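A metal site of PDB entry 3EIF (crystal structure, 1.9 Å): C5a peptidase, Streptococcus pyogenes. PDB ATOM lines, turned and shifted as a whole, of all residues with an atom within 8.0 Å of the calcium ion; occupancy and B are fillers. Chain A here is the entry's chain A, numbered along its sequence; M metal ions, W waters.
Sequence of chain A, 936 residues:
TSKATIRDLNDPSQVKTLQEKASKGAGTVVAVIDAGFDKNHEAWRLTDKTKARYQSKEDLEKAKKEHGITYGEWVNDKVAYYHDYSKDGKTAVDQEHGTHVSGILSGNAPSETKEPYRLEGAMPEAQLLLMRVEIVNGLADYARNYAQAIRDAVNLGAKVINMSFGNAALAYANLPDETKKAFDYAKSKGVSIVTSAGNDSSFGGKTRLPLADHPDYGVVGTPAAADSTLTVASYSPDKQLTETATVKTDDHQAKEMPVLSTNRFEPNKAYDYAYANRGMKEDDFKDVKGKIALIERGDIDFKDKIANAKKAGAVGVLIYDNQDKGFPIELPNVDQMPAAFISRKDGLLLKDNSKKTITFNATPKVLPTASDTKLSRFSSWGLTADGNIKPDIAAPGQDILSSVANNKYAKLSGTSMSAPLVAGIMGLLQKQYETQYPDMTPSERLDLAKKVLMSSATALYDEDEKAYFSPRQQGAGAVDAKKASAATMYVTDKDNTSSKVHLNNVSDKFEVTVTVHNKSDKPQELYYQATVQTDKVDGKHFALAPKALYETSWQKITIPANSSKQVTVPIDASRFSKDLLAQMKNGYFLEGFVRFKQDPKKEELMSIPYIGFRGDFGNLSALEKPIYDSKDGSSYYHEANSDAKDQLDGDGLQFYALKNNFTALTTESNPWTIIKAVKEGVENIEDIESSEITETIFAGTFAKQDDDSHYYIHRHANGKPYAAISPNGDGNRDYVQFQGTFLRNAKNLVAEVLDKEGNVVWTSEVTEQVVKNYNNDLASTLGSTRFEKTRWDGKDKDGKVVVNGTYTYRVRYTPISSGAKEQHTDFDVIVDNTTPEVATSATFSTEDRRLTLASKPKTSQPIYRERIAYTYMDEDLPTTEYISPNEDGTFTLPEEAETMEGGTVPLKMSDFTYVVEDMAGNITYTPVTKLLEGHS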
ATOM      1  N   GLU A 668     -15.386  -1.081   7.209  1.00  0.00           N
ATOM      2  CA  GLU A 668     -14.964   0.290   7.419  1.00  0.00           C
ATOM      3  C   GLU A 668     -13.702   0.678   6.631  1.00  0.00           C
ATOM      4  O   GLU A 668     -12.802  -0.138   6.431  1.00  0.00           O
ATOM      5  CB  GLU A 668     -14.724   0.566   8.916  1.00  0.00           C
ATOM      6  CG  GLU A 668     -16.012   0.621   9.728  1.00  0.00           C
ATOM      7  CD  GLU A 668     -15.778   0.730  11.218  1.00  0.00           C
ATOM      8  OE1 GLU A 668     -14.890   1.504  11.645  1.00  0.00           O
ATOM      9  OE2 GLU A 668     -16.504   0.047  11.972  1.00  0.00           O
ATOM     10  N   ASN A 670     -10.521   3.054   6.650  1.00  0.00           N
ATOM     11  CA  ASN A 670      -9.714   3.835   7.570  1.00  0.00           C
ATOM     12  C   ASN A 670      -8.546   4.380   6.751  1.00  0.00           C
ATOM     13  O   ASN A 670      -7.659   3.638   6.340  1.00  0.00           O
ATOM     14  CB  ASN A 670      -9.188   2.959   8.718  1.00  0.00           C
ATOM     15  CG  ASN A 670      -8.933   3.760   9.975  1.00  0.00           C
ATOM     16  OD1 ASN A 670      -9.314   4.926  10.045  1.00  0.00           O
ATOM     17  ND2 ASN A 670      -8.308   3.141  10.977  1.00  0.00           N
ATOM     18  N   ILE A 675      -4.714   5.755  10.354  1.00  0.00           N
ATOM     19  CA  ILE A 675      -4.021   4.533  10.736  1.00  0.00           C
ATOM     20  C   ILE A 675      -2.681   4.939  11.382  1.00  0.00           C
ATOM     21  O   ILE A 675      -2.318   4.445  12.446  1.00  0.00           O
ATOM     22  CB  ILE A 675      -3.728   3.646   9.495  1.00  0.00           C
ATOM     23  CG1 ILE A 675      -5.044   3.118   8.905  1.00  0.00           C
ATOM     24  CG2 ILE A 675      -2.850   2.463   9.911  1.00  0.00           C
ATOM     25  CD1 ILE A 675      -4.859   2.277   7.627  1.00  0.00           C
ATOM     26  N   ALA A 724     -13.706  -8.120   0.395  1.00  0.00           N
ATOM     27  CA  ALA A 724     -12.401  -8.613   0.827  1.00  0.00           C
ATOM     28  C   ALA A 724     -11.979  -7.900   2.112  1.00  0.00           C
ATOM     29  O   ALA A 724     -12.235  -6.705   2.276  1.00  0.00           O
ATOM     30  CB  ALA A 724     -11.340  -8.378  -0.277  1.00  0.00           C
ATOM     31  N   ILE A 725     -11.354  -8.629   3.022  1.00  0.00           N
ATOM     32  CA  ILE A 725     -10.884  -8.041   4.268  1.00  0.00           C
ATOM     33  C   ILE A 725      -9.406  -8.384   4.545  1.00  0.00           C
ATOM     34  O   ILE A 725      -8.883  -9.388   4.058  1.00  0.00           O
ATOM     35  CB  ILE A 725     -11.735  -8.510   5.483  1.00  0.00           C
ATOM     36  CG1 ILE A 725     -11.690 -10.041   5.597  1.00  0.00           C
ATOM     37  CG2 ILE A 725     -13.171  -8.003   5.346  1.00  0.00           C
ATOM     38  CD1 ILE A 725     -12.416 -10.567   6.855  1.00  0.00           C
ATOM     39  N   SER A 726      -8.744  -7.505   5.294  1.00  0.00           N
ATOM     40  CA  SER A 726      -7.337  -7.680   5.688  1.00  0.00           C
ATOM     41  C   SER A 726      -7.370  -7.639   7.218  1.00  0.00           C
ATOM     42  O   SER A 726      -7.173  -6.592   7.813  1.00  0.00           O
ATOM     43  CB  SER A 726      -6.473  -6.547   5.133  1.00  0.00           C
ATOM     44  OG  SER A 726      -7.134  -5.293   5.217  1.00  0.00           O
ATOM     45  N   PRO A 727      -7.628  -8.766   7.872  1.00  0.00           N
ATOM     46  CA  PRO A 727      -7.685  -8.766   9.347  1.00  0.00           C
ATOM     47  C   PRO A 727      -6.352  -8.557  10.063  1.00  0.00           C
ATOM     48  O   PRO A 727      -5.794  -9.474  10.637  1.00  0.00           O
ATOM     49  CB  PRO A 727      -8.327 -10.123   9.657  1.00  0.00           C
ATOM     50  CG  PRO A 727      -7.773 -10.993   8.574  1.00  0.00           C
ATOM     51  CD  PRO A 727      -7.875 -10.117   7.335  1.00  0.00           C
ATOM     52  N   ASN A 728      -5.861  -7.325  10.036  1.00  0.00           N
ATOM     53  CA  ASN A 728      -4.588  -6.996  10.671  1.00  0.00           C
ATOM     54  C   ASN A 728      -4.718  -5.902  11.713  1.00  0.00           C
ATOM     55  O   ASN A 728      -3.734  -5.279  12.107  1.00  0.00           O
ATOM     56  CB  ASN A 728      -3.572  -6.594   9.604  1.00  0.00           C
ATOM     57  CG  ASN A 728      -4.076  -5.473   8.739  1.00  0.00           C
ATOM     58  OD1 ASN A 728      -5.003  -4.774   9.124  1.00  0.00           O
ATOM     59  ND2 ASN A 728      -3.466  -5.291   7.578  1.00  0.00           N
ATOM     60  N   GLY A 729      -5.950  -5.650  12.161  1.00  0.00           N
ATOM     61  CA  GLY A 729      -6.203  -4.675  13.209  1.00  0.00           C
ATOM     62  C   GLY A 729      -6.013  -3.189  12.991  1.00  0.00           C
ATOM     63  O   GLY A 729      -6.029  -2.446  13.978  1.00  0.00           O
ATOM     64  N   ASP A 730      -5.852  -2.716  11.746  1.00  0.00           N
ATOM     65  CA  ASP A 730      -5.678  -1.279  11.529  1.00  0.00           C
ATOM     66  C   ASP A 730      -6.995  -0.538  11.289  1.00  0.00           C
ATOM     67  O   ASP A 730      -7.010   0.668  11.045  1.00  0.00           O
ATOM     68  CB  ASP A 730      -4.695  -1.013  10.372  1.00  0.00           C
ATOM     69  CG  ASP A 730      -5.190  -1.541   9.035  1.00  0.00           C
ATOM     70  OD1 ASP A 730      -4.425  -1.447   8.043  1.00  0.00           O
ATOM     71  OD2 ASP A 730      -6.344  -2.040   8.961  1.00  0.00           O
ATOM     72  N   GLY A 731      -8.110  -1.265  11.368  1.00  0.00           N
ATOM     73  CA  GLY A 731      -9.403  -0.634  11.175  1.00  0.00           C
ATOM     74  C   GLY A 731      -9.791  -0.409   9.729  1.00  0.00           C
ATOM     75  O   GLY A 731     -10.888   0.100   9.442  1.00  0.00           O
ATOM     76  N   ASN A 732      -8.897  -0.748   8.808  1.00  0.00           N
ATOM     77  CA  ASN A 732      -9.196  -0.557   7.393  1.00  0.00           C
ATOM     78  C   ASN A 732      -9.643  -1.882   6.809  1.00  0.00           C
ATOM     79  O   ASN A 732      -8.849  -2.780   6.635  1.00  0.00           O
ATOM     80  CB  ASN A 732      -7.960  -0.039   6.649  1.00  0.00           C
ATOM     81  CG  ASN A 732      -8.263   0.352   5.199  1.00  0.00           C
ATOM     82  OD1 ASN A 732      -9.278   0.999   4.916  1.00  0.00           O
ATOM     83  ND2 ASN A 732      -7.367  -0.024   4.285  1.00  0.00           N
ATOM     84  N   ARG A 733     -10.926  -1.993   6.501  1.00  0.00           N
ATOM     85  CA  ARG A 733     -11.475  -3.220   5.915  1.00  0.00           C
ATOM     86  C   ARG A 733     -11.057  -4.491   6.685  1.00  0.00           C
ATOM     87  O   ARG A 733     -10.598  -5.477   6.081  1.00  0.00           O
ATOM     88  CB  ARG A 733     -11.062  -3.289   4.437  1.00  0.00           C
ATOM     89  CG  ARG A 733     -11.693  -2.165   3.592  1.00  0.00           C
ATOM     90  CD  ARG A 733     -11.042  -1.992   2.195  1.00  0.00           C
ATOM     91  NE  ARG A 733     -11.587  -0.808   1.502  1.00  0.00           N
ATOM     92  CZ  ARG A 733     -12.643  -0.802   0.688  1.00  0.00           C
ATOM     93  NH1 ARG A 733     -13.314  -1.933   0.427  1.00  0.00           N
ATOM     94  NH2 ARG A 733     -13.052   0.341   0.151  1.00  0.00           N
ATOM     95  N   ASP A 734     -11.221  -4.466   8.003  1.00  0.00           N
ATOM     96  CA  ASP A 734     -10.861  -5.584   8.889  1.00  0.00           C
ATOM     97  C   ASP A 734     -11.966  -6.622   9.052  1.00  0.00           C
ATOM     98  O   ASP A 734     -11.698  -7.766   9.433  1.00  0.00           O
ATOM     99  CB  ASP A 734     -10.535  -5.075  10.312  1.00  0.00           C
ATOM    100  CG  ASP A 734      -9.180  -4.372  10.405  1.00  0.00           C
ATOM    101  OD1 ASP A 734      -8.484  -4.318   9.382  1.00  0.00           O
ATOM    102  OD2 ASP A 734      -8.811  -3.869  11.501  1.00  0.00           O
ATOM    103  N   TYR A 735     -13.209  -6.237   8.750  1.00  0.00           N
ATOM    104  CA  TYR A 735     -14.316  -7.165   8.963  1.00  0.00           C
ATOM    105  C   TYR A 735     -15.469  -6.938   7.992  1.00  0.00           C
ATOM    106  O   TYR A 735     -15.471  -5.979   7.215  1.00  0.00           O
ATOM    107  CB  TYR A 735     -14.839  -6.978  10.390  1.00  0.00           C
ATOM    108  CG  TYR A 735     -15.578  -5.662  10.591  1.00  0.00           C
ATOM    109  CD1 TYR A 735     -16.905  -5.525  10.165  1.00  0.00           C
ATOM    110  CD2 TYR A 735     -14.961  -4.559  11.166  1.00  0.00           C
ATOM    111  CE1 TYR A 735     -17.585  -4.324  10.299  1.00  0.00           C
ATOM    112  CE2 TYR A 735     -15.636  -3.342  11.314  1.00  0.00           C
ATOM    113  CZ  TYR A 735     -16.956  -3.238  10.874  1.00  0.00           C
ATOM    114  OH  TYR A 735     -17.647  -2.058  11.002  1.00  0.00           O
ATOM    115  N   ASP A 832      -7.214 -11.606   2.890  1.00  0.00           N
ATOM    116  CA  ASP A 832      -5.835 -11.480   2.415  1.00  0.00           C
ATOM    117  C   ASP A 832      -5.126 -10.457   3.297  1.00  0.00           C
ATOM    118  O   ASP A 832      -5.504  -9.274   3.325  1.00  0.00           O
ATOM    119  CB  ASP A 832      -5.794 -11.015   0.956  1.00  0.00           C
ATOM    120  CG  ASP A 832      -4.433 -11.248   0.325  1.00  0.00           C
ATOM    121  OD1 ASP A 832      -3.415 -10.911   0.957  1.00  0.00           O
ATOM    122  OD2 ASP A 832      -4.388 -11.748  -0.825  1.00  0.00           O
ATOM    123  N   ASN A 833      -4.120 -10.926   4.034  1.00  0.00           N
ATOM    124  CA  ASN A 833      -3.368 -10.072   4.943  1.00  0.00           C
ATOM    125  C   ASN A 833      -1.983  -9.725   4.411  1.00  0.00           C
ATOM    126  O   ASN A 833      -1.127  -9.252   5.157  1.00  0.00           O
ATOM    127  CB  ASN A 833      -3.203 -10.779   6.299  1.00  0.00           C
ATOM    128  CG  ASN A 833      -4.024 -10.152   7.401  1.00  0.00           C
ATOM    129  OD1 ASN A 833      -4.137 -10.708   8.495  1.00  0.00           O
ATOM    130  ND2 ASN A 833      -4.590  -8.974   7.127  1.00  0.00           N
ATOM    131  N   GLU A 917      -2.385   0.907  -1.589  1.00  0.00           N
ATOM    132  CA  GLU A 917      -3.413   0.098  -0.963  1.00  0.00           C
ATOM    133  C   GLU A 917      -3.965  -0.939  -1.944  1.00  0.00           C
ATOM    134  O   GLU A 917      -4.148  -0.643  -3.131  1.00  0.00           O
ATOM    135  CB  GLU A 917      -4.531   1.040  -0.504  1.00  0.00           C
ATOM    136  CG  GLU A 917      -5.693   0.402   0.236  1.00  0.00           C
ATOM    137  CD  GLU A 917      -6.733   1.404   0.677  1.00  0.00           C
ATOM    138  OE1 GLU A 917      -6.772   2.516   0.101  1.00  0.00           O
ATOM    139  OE2 GLU A 917      -7.523   1.081   1.584  1.00  0.00           O
ATOM    140  N   ALA A 920      -7.965  -5.528  -0.578  1.00  0.00           N
ATOM    141  CA  ALA A 920      -8.393  -6.092   0.708  1.00  0.00           C
ATOM    142  C   ALA A 920      -8.139  -5.033   1.775  1.00  0.00           C
ATOM    143  O   ALA A 920      -8.458  -5.222   2.951  1.00  0.00           O
ATOM    144  CB  ALA A 920      -7.608  -7.356   1.036  1.00  0.00           C
ATOM    145  N   GLY A 921      -7.552  -3.915   1.368  1.00  0.00           N
ATOM    146  CA  GLY A 921      -7.256  -2.859   2.326  1.00  0.00           C
ATOM    147  C   GLY A 921      -5.844  -2.912   2.918  1.00  0.00           C
ATOM    148  O   GLY A 921      -5.528  -2.152   3.839  1.00  0.00           O
ATOM    149  N   ASN A 922      -4.995  -3.818   2.423  1.00  0.00           N
ATOM    150  CA  ASN A 922      -3.622  -3.872   2.931  1.00  0.00           C
ATOM    151  C   ASN A 922      -2.999  -2.585   2.430  1.00  0.00           C
ATOM    152  O   ASN A 922      -3.200  -2.215   1.273  1.00  0.00           O
ATOM    153  CB  ASN A 922      -2.902  -5.102   2.384  1.00  0.00           C
ATOM    154  CG  ASN A 922      -3.411  -6.369   3.007  1.00  0.00           C
ATOM    155  OD1 ASN A 922      -3.225  -6.600   4.194  1.00  0.00           O
ATOM    156  ND2 ASN A 922      -4.095  -7.187   2.209  1.00  0.00           N
ATOM    157  N   ILE A 923      -2.214  -1.930   3.273  1.00  0.00           N
ATOM    158  CA  ILE A 923      -1.695  -0.627   2.898  1.00  0.00           C
ATOM    159  C   ILE A 923      -0.306  -0.280   3.449  1.00  0.00           C
ATOM    160  O   ILE A 923       0.086  -0.765   4.512  1.00  0.00           O
ATOM    161  CB  ILE A 923      -2.712   0.416   3.380  1.00  0.00           C
ATOM    162  CG1 ILE A 923      -2.339   1.825   2.934  1.00  0.00           C
ATOM    163  CG2 ILE A 923      -2.829   0.357   4.900  1.00  0.00           C
ATOM    164  CD1 ILE A 923      -3.465   2.816   3.266  1.00  0.00           C
HETATM  165 CA    CA M   1      -6.998  -4.085   7.585  1.00  0.00          CA
HETATM  166  O   HOH W   1      -5.041  -3.133   6.277  1.00  0.00           O
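The side-chain carboxylate (OD2) of Asp 734 lies within hydrogen-bond range of the backbone NH (N) of Gly 731 (2.7 Å).
The side-chain carboxylate (OD2) of Asp 734 sits close to the backbone NH (N) of Gly 729.
ND2 of Asn 732 lies within hydrogen-bond range of O of Gly 921, at 2.8 Å.
OD1 of Asn 732 is in hydrogen-bond range of N of Asn 670.
The side-chain amide nitrogen (ND2) of Asn 732 sits at hydrogen-bond distance from the side-chain carboxylate (OE2) of Glu 917, 2.9 Å away.
The backbone carbonyl oxygen of Arg 733 sits at hydrogen-bond distance from the backbone NH of Ser 726 (2.9 Å).
N of Ser 726 sits close to O of Ala 920 (3.3 Å).
The backbone carbonyl oxygen (O) of Asp 730 lies within hydrogen-bond range of the side-chain amide nitrogen (ND2) of Asn 670 (2.8 Å).
Of the 22 residues printed, 5 come within 4 Å of the calcium ion.
OD1 of Asp 734 binds the calcium ion (2.3 Å).
The calcium ion is bound by the backbone carbonyl oxygen (O) of Asn 732 (2.5 Å).
O of Ser 726 binds the calcium ion (2.5 Å).
Water W1 is bound to the calcium ion.
OD2 of Asp 730 is bound to the calcium ion.
OD1 of Asn 728 is bound to the calcium ion, 2.6 Å away.
OG of Ser 726 is bound to the calcium ion (2.7 Å).
The calcium ion has seven donor atoms within binding distance.
Water W1 lies within hydrogen-bond range of OD1 of Asp 730 (2.5 Å), O of Gly 921 (2.7 Å) and ND2 of Asn 728 (3.0 Å).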
